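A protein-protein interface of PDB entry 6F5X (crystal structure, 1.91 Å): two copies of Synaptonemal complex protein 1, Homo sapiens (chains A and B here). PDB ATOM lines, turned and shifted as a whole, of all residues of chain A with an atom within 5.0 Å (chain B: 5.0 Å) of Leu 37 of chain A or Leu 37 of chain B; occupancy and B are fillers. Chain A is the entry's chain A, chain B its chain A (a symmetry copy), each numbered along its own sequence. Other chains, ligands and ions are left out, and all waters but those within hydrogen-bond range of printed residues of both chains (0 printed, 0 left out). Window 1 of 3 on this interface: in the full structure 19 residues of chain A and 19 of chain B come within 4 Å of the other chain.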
ATOM      1  N   GLN A  32      10.715  32.453  -2.541  1.00  0.00           N
ATOM      2  CA  GLN A  32      10.774  31.177  -3.246  1.00  0.00           C
ATOM      3  C   GLN A  32      10.172  30.043  -2.422  1.00  0.00           C
ATOM      4  O   GLN A  32       9.438  29.200  -2.962  1.00  0.00           O
ATOM      5  CB  GLN A  32      12.207  30.872  -3.657  1.00  0.00           C
ATOM      6  CG  GLN A  32      12.670  31.843  -4.708  1.00  0.00           C
ATOM      7  CD  GLN A  32      11.751  31.814  -5.919  1.00  0.00           C
ATOM      8  OE1 GLN A  32      11.018  32.772  -6.177  1.00  0.00           O
ATOM      9  NE2 GLN A  32      11.759  30.699  -6.645  1.00  0.00           N
ATOM     10  N   LYS A  33      10.452  30.010  -1.116  1.00  0.00           N
ATOM     11  CA  LYS A  33       9.841  28.993  -0.264  1.00  0.00           C
ATOM     12  C   LYS A  33       8.332  29.144  -0.223  1.00  0.00           C
ATOM     13  O   LYS A  33       7.605  28.153  -0.327  1.00  0.00           O
ATOM     14  CB  LYS A  33      10.412  29.057   1.153  1.00  0.00           C
ATOM     15  CG  LYS A  33      11.856  28.637   1.258  1.00  0.00           C
ATOM     16  CD  LYS A  33      12.320  28.671   2.696  1.00  0.00           C
ATOM     17  CE  LYS A  33      13.792  28.352   2.784  1.00  0.00           C
ATOM     18  NZ  LYS A  33      14.067  26.947   2.398  1.00  0.00           N
ATOM     19  N   GLU A  34       7.844  30.377  -0.069  1.00  0.00           N
ATOM     20  CA  GLU A  34       6.404  30.629  -0.064  1.00  0.00           C
ATOM     21  C   GLU A  34       5.767  30.204  -1.384  1.00  0.00           C
ATOM     22  O   GLU A  34       4.723  29.534  -1.404  1.00  0.00           O
ATOM     23  CB  GLU A  34       6.147  32.112   0.216  1.00  0.00           C
ATOM     24  CG  GLU A  34       4.685  32.491   0.283  1.00  0.00           C
ATOM     25  CD  GLU A  34       3.971  31.840   1.451  1.00  0.00           C
ATOM     26  OE1 GLU A  34       4.650  31.529   2.454  1.00  0.00           O
ATOM     27  OE2 GLU A  34       2.738  31.633   1.367  1.00  0.00           O
ATOM     28  N   SER A  35       6.390  30.589  -2.500  1.00  0.00           N
ATOM     29  CA  SER A  35       5.916  30.172  -3.815  1.00  0.00           C
ATOM     30  C   SER A  35       5.772  28.655  -3.896  1.00  0.00           C
ATOM     31  O   SER A  35       4.709  28.134  -4.269  1.00  0.00           O
ATOM     32  CB  SER A  35       6.875  30.695  -4.888  1.00  0.00           C
ATOM     33  OG  SER A  35       6.478  30.294  -6.189  1.00  0.00           O
ATOM     34  N   LYS A  36       6.827  27.924  -3.520  1.00  0.00           N
ATOM     35  CA  LYS A  36       6.770  26.470  -3.647  1.00  0.00           C
ATOM     36  C   LYS A  36       5.850  25.831  -2.612  1.00  0.00           C
ATOM     37  O   LYS A  36       5.278  24.773  -2.884  1.00  0.00           O
ATOM     38  CB  LYS A  36       8.178  25.872  -3.591  1.00  0.00           C
ATOM     39  CG  LYS A  36       9.028  26.251  -4.809  1.00  0.00           C
ATOM     40  CD  LYS A  36       8.442  25.598  -6.070  1.00  0.00           C
ATOM     41  CE  LYS A  36       9.283  25.798  -7.330  1.00  0.00           C
ATOM     42  NZ  LYS A  36       9.243  27.195  -7.832  1.00  0.00           N
ATOM     43  N   LEU A  37       5.673  26.450  -1.441  1.00  0.00           N
ATOM     44  CA  LEU A  37       4.631  26.001  -0.521  1.00  0.00           C
ATOM     45  C   LEU A  37       3.256  26.104  -1.157  1.00  0.00           C
ATOM     46  O   LEU A  37       2.478  25.153  -1.114  1.00  0.00           O
ATOM     47  CB  LEU A  37       4.662  26.797   0.782  1.00  0.00           C
ATOM     48  CG  LEU A  37       5.740  26.576   1.837  1.00  0.00           C
ATOM     49  CD1 LEU A  37       5.604  27.635   2.886  1.00  0.00           C
ATOM     50  CD2 LEU A  37       5.497  25.235   2.475  1.00  0.00           C
ATOM     51  N   GLN A  38       2.933  27.256  -1.750  1.00  0.00           N
ATOM     52  CA  GLN A  38       1.634  27.408  -2.404  1.00  0.00           C
ATOM     53  C   GLN A  38       1.440  26.344  -3.481  1.00  0.00           C
ATOM     54  O   GLN A  38       0.384  25.692  -3.552  1.00  0.00           O
ATOM     55  CB  GLN A  38       1.497  28.818  -2.989  1.00  0.00           C
ATOM     56  CG  GLN A  38       0.117  29.112  -3.594  1.00  0.00           C
ATOM     57  CD  GLN A  38      -0.039  30.549  -4.087  1.00  0.00           C
ATOM     58  OE1 GLN A  38       0.900  31.346  -4.025  1.00  0.00           O
ATOM     59  NE2 GLN A  38      -1.234  30.886  -4.572  1.00  0.00           N
ATOM     60  N   GLU A  39       2.467  26.135  -4.316  1.00  0.00           N
ATOM     61  CA  GLU A  39       2.427  25.015  -5.254  1.00  0.00           C
ATOM     62  C   GLU A  39       2.124  23.697  -4.537  1.00  0.00           C
ATOM     63  O   GLU A  39       1.313  22.881  -5.014  1.00  0.00           O
ATOM     64  CB  GLU A  39       3.754  24.921  -6.016  1.00  0.00           C
ATOM     65  CG  GLU A  39       3.790  23.806  -7.072  1.00  0.00           C
ATOM     66  CD  GLU A  39       5.098  23.743  -7.856  1.00  0.00           C
ATOM     67  OE1 GLU A  39       6.000  24.561  -7.582  1.00  0.00           O
ATOM     68  OE2 GLU A  39       5.227  22.867  -8.743  1.00  0.00           O
ATOM     69  N   ASN A  40       2.756  23.475  -3.377  1.00  0.00           N
ATOM     70  CA  ASN A  40       2.550  22.222  -2.659  1.00  0.00           C
ATOM     71  C   ASN A  40       1.107  22.074  -2.208  1.00  0.00           C
ATOM     72  O   ASN A  40       0.534  20.984  -2.302  1.00  0.00           O
ATOM     73  CB  ASN A  40       3.471  22.111  -1.448  1.00  0.00           C
ATOM     74  CG  ASN A  40       4.914  21.913  -1.823  1.00  0.00           C
ATOM     75  OD1 ASN A  40       5.227  21.257  -2.813  1.00  0.00           O
ATOM     76  ND2 ASN A  40       5.807  22.397  -0.977  1.00  0.00           N
ATOM     77  N   ARG A  41       0.511  23.147  -1.678  1.00  0.00           N
ATOM     78  CA  ARG A  41      -0.887  23.053  -1.275  1.00  0.00           C
ATOM     79  C   ARG A  41      -1.767  22.678  -2.457  1.00  0.00           C
ATOM     80  O   ARG A  41      -2.670  21.839  -2.325  1.00  0.00           O
ATOM     81  CB  ARG A  41      -1.362  24.354  -0.630  1.00  0.00           C
ATOM     82  CG  ARG A  41      -0.976  24.507   0.834  1.00  0.00           C
ATOM     83  CD  ARG A  41       0.381  25.162   1.009  1.00  0.00           C
ATOM     84  NE  ARG A  41       0.646  25.544   2.397  1.00  0.00           N
ATOM     85  CZ  ARG A  41       1.310  24.792   3.268  1.00  0.00           C
ATOM     86  NH1 ARG A  41       1.787  23.611   2.895  1.00  0.00           N
ATOM     87  NH2 ARG A  41       1.499  25.219   4.508  1.00  0.00           N
ATOM     88  N   GLN B  32      10.705  27.435   9.850  1.00  0.00           N
ATOM     89  CA  GLN B  32       9.334  26.937   9.835  1.00  0.00           C
ATOM     90  C   GLN B  32       8.860  26.615   8.421  1.00  0.00           C
ATOM     91  O   GLN B  32       8.207  25.584   8.201  1.00  0.00           O
ATOM     92  CB  GLN B  32       8.409  27.929  10.525  1.00  0.00           C
ATOM     93  CG  GLN B  32       8.713  27.995  11.996  1.00  0.00           C
ATOM     94  CD  GLN B  32       8.595  26.622  12.639  1.00  0.00           C
ATOM     95  OE1 GLN B  32       9.597  26.027  13.044  1.00  0.00           O
ATOM     96  NE2 GLN B  32       7.375  26.097  12.699  1.00  0.00           N
ATOM     97  N   LYS B  33       9.188  27.471   7.449  1.00  0.00           N
ATOM     98  CA  LYS B  33       8.828  27.176   6.064  1.00  0.00           C
ATOM     99  C   LYS B  33       9.518  25.917   5.574  1.00  0.00           C
ATOM    100  O   LYS B  33       8.887  25.072   4.933  1.00  0.00           O
ATOM    101  CB  LYS B  33       9.174  28.351   5.150  1.00  0.00           C
ATOM    102  CG  LYS B  33       8.327  29.578   5.372  1.00  0.00           C
ATOM    103  CD  LYS B  33       8.693  30.666   4.389  1.00  0.00           C
ATOM    104  CE  LYS B  33       7.917  31.927   4.683  1.00  0.00           C
ATOM    105  NZ  LYS B  33       6.468  31.745   4.425  1.00  0.00           N
ATOM    106  N   GLU B  34      10.813  25.775   5.862  1.00  0.00           N
ATOM    107  CA  GLU B  34      11.552  24.575   5.474  1.00  0.00           C
ATOM    108  C   GLU B  34      10.952  23.328   6.115  1.00  0.00           C
ATOM    109  O   GLU B  34      10.742  22.303   5.447  1.00  0.00           O
ATOM    110  CB  GLU B  34      13.024  24.736   5.860  1.00  0.00           C
ATOM    111  CG  GLU B  34      13.904  23.568   5.473  1.00  0.00           C
ATOM    112  CD  GLU B  34      14.008  23.395   3.970  1.00  0.00           C
ATOM    113  OE1 GLU B  34      13.845  24.405   3.251  1.00  0.00           O
ATOM    114  OE2 GLU B  34      14.244  22.255   3.508  1.00  0.00           O
ATOM    115  N   SER B  35      10.668  23.402   7.417  1.00  0.00           N
ATOM    116  CA  SER B  35      10.019  22.299   8.116  1.00  0.00           C
ATOM    117  C   SER B  35       8.731  21.881   7.412  1.00  0.00           C
ATOM    118  O   SER B  35       8.533  20.697   7.093  1.00  0.00           O
ATOM    119  CB  SER B  35       9.748  22.707   9.567  1.00  0.00           C
ATOM    120  OG  SER B  35       9.089  21.680  10.288  1.00  0.00           O
ATOM    121  N   LYS B  36       7.851  22.847   7.132  1.00  0.00           N
ATOM    122  CA  LYS B  36       6.569  22.493   6.525  1.00  0.00           C
ATOM    123  C   LYS B  36       6.712  22.080   5.063  1.00  0.00           C
ATOM    124  O   LYS B  36       5.909  21.279   4.581  1.00  0.00           O
ATOM    125  CB  LYS B  36       5.564  23.635   6.690  1.00  0.00           C
ATOM    126  CG  LYS B  36       5.158  23.857   8.151  1.00  0.00           C
ATOM    127  CD  LYS B  36       4.363  22.642   8.655  1.00  0.00           C
ATOM    128  CE  LYS B  36       3.791  22.806  10.062  1.00  0.00           C
ATOM    129  NZ  LYS B  36       4.837  22.768  11.116  1.00  0.00           N
ATOM    130  N   LEU B  37       7.721  22.586   4.349  1.00  0.00           N
ATOM    131  CA  LEU B  37       8.032  22.047   3.028  1.00  0.00           C
ATOM    132  C   LEU B  37       8.394  20.574   3.109  1.00  0.00           C
ATOM    133  O   LEU B  37       7.867  19.762   2.350  1.00  0.00           O
ATOM    134  CB  LEU B  37       9.165  22.825   2.363  1.00  0.00           C
ATOM    135  CG  LEU B  37       8.956  24.219   1.784  1.00  0.00           C
ATOM    136  CD1 LEU B  37      10.287  24.778   1.391  1.00  0.00           C
ATOM    137  CD2 LEU B  37       8.108  24.085   0.548  1.00  0.00           C
ATOM    138  N   GLN B  38       9.298  20.208   4.020  1.00  0.00           N
ATOM    139  CA  GLN B  38       9.669  18.801   4.165  1.00  0.00           C
ATOM    140  C   GLN B  38       8.441  17.944   4.463  1.00  0.00           C
ATOM    141  O   GLN B  38       8.234  16.887   3.841  1.00  0.00           O
ATOM    142  CB  GLN B  38      10.732  18.643   5.258  1.00  0.00           C
ATOM    143  CG  GLN B  38      11.272  17.213   5.402  1.00  0.00           C
ATOM    144  CD  GLN B  38      12.397  17.087   6.427  1.00  0.00           C
ATOM    145  OE1 GLN B  38      12.768  18.062   7.083  1.00  0.00           O
ATOM    146  NE2 GLN B  38      12.950  15.881   6.559  1.00  0.00           N
ATOM    147  N   GLU B  39       7.598  18.400   5.398  1.00  0.00           N
ATOM    148  CA  GLU B  39       6.315  17.732   5.611  1.00  0.00           C
ATOM    149  C   GLU B  39       5.537  17.589   4.300  1.00  0.00           C
ATOM    150  O   GLU B  39       4.958  16.524   4.015  1.00  0.00           O
ATOM    151  CB  GLU B  39       5.488  18.502   6.647  1.00  0.00           C
ATOM    152  CG  GLU B  39       4.142  17.845   6.984  1.00  0.00           C
ATOM    153  CD  GLU B  39       3.341  18.594   8.046  1.00  0.00           C
ATOM    154  OE1 GLU B  39       3.819  19.641   8.528  1.00  0.00           O
ATOM    155  OE2 GLU B  39       2.226  18.137   8.393  1.00  0.00           O
ATOM    156  N   ASN B  40       5.524  18.646   3.481  1.00  0.00           N
ATOM    157  CA  ASN B  40       4.766  18.597   2.234  1.00  0.00           C
ATOM    158  C   ASN B  40       5.318  17.539   1.293  1.00  0.00           C
ATOM    159  O   ASN B  40       4.549  16.816   0.652  1.00  0.00           O
ATOM    160  CB  ASN B  40       4.764  19.949   1.526  1.00  0.00           C
ATOM    161  CG  ASN B  40       3.940  20.985   2.242  1.00  0.00           C
ATOM    162  OD1 ASN B  40       2.913  20.676   2.840  1.00  0.00           O
ATOM    163  ND2 ASN B  40       4.332  22.240   2.100  1.00  0.00           N
ATOM    164  N   ARG B  41       6.646  17.456   1.165  1.00  0.00           N
ATOM    165  CA  ARG B  41       7.210  16.424   0.305  1.00  0.00           C
ATOM    166  C   ARG B  41       6.789  15.039   0.774  1.00  0.00           C
ATOM    167  O   ARG B  41       6.436  14.180  -0.047  1.00  0.00           O
ATOM    168  CB  ARG B  41       8.732  16.537   0.234  1.00  0.00           C
ATOM    169  CG  ARG B  41       9.238  17.591  -0.740  1.00  0.00           C
ATOM    170  CD  ARG B  41       9.376  18.957  -0.096  1.00  0.00           C
ATOM    171  NE  ARG B  41      10.097  19.908  -0.942  1.00  0.00           N
ATOM    172  CZ  ARG B  41       9.512  20.768  -1.770  1.00  0.00           C
ATOM    173  NH1 ARG B  41       8.189  20.805  -1.861  1.00  0.00           N
ATOM    174  NH2 ARG B  41      10.248  21.592  -2.504  1.00  0.00           N
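The side-chain amino group (NZ) of Lys 33 of chain A lies within salt-bridge range of the side-chain carboxylate (OE1) of Glu 34 of chain B (2.7 Å). The side-chain carboxylate (OE1) of Glu 34 of chain A is in salt-bridge range of the side-chain amino group (NZ) of Lys 33 of chain B, at 2.7 Å. ND2 of Asn 40 of chain A lies close to ND2 of Asn 40 of chain B (3.4 Å). The side-chain amide nitrogen (ND2) of Asn 40 of chain A lies close to the guanidinium group (NH1) of Arg 41 of chain B (3.0 Å). NH1 of Arg 41 of chain A lies close to ND2 of Asn 40 of chain B (3.0 Å).
The backbone carbonyl oxygen of Lys 36 of chain A lies close to the side-chain amide nitrogen of Asn 40 of chain A. The side-chain amide nitrogen of Asn 40 of chain B sits close to the backbone carbonyl oxygen of Lys 36 of chain B, at 3.1 Å.
CD2 of Leu 37 of chain A touches CD2 of Leu 37 of chain B (3.4 Å). CD2 of Leu 37 of chain A touches ND2 of Asn 40 of chain B (3.2 Å). Asn 40 of chain A touches Leu 37 of chain B (ND2 to CD2, 3.2 Å).
Leu 37 of chain A touches two residues of chain B. Of chain A, only Leu 37 and Asn 40 come within 4 Å of Leu 37 of chain B. Of the printed residues of chain B, Arg 41 of chain A touches Asn 40 (3.0 Å). Printed residues of chain A within 4 Å of Glu 34 of chain B: Lys 33 (2.7 Å). Printed residues of chain B within 4 Å of Asn 40 of chain A: Leu 37 (3.2 Å), Asn 40 (3.4 Å) and Arg 41 (3.0 Å). The nearest residue of chain A that does not touch Leu 37 of chain B is Lys 33 of chain A (4.2 Å).
Hydrophobic or aromatic side chains of chain A within 4 Å of the printed part of chain B: Leu 37. Hydrophobic or aromatic side chains of chain B within 4 Å of the printed part of chain A: Leu 37.
Lys 33 of chain A touches Glu 34 of chain B, and with the chains exchanged Glu 34 of chain A touches Lys 33 of chain B. Leu 37 of chain A touches its own counterpart, Leu 37 of chain B. Leu 37 of chain A touches Asn 40 of chain B, and with the chains exchanged Asn 40 of chain A touches Leu 37 of chain B. Asn 40 of chain A touches its own counterpart, Asn 40 of chain B. Of the 8 pairs that touch across the chains among the printed residues, 8 have their exchanged pair printed and touching as well.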
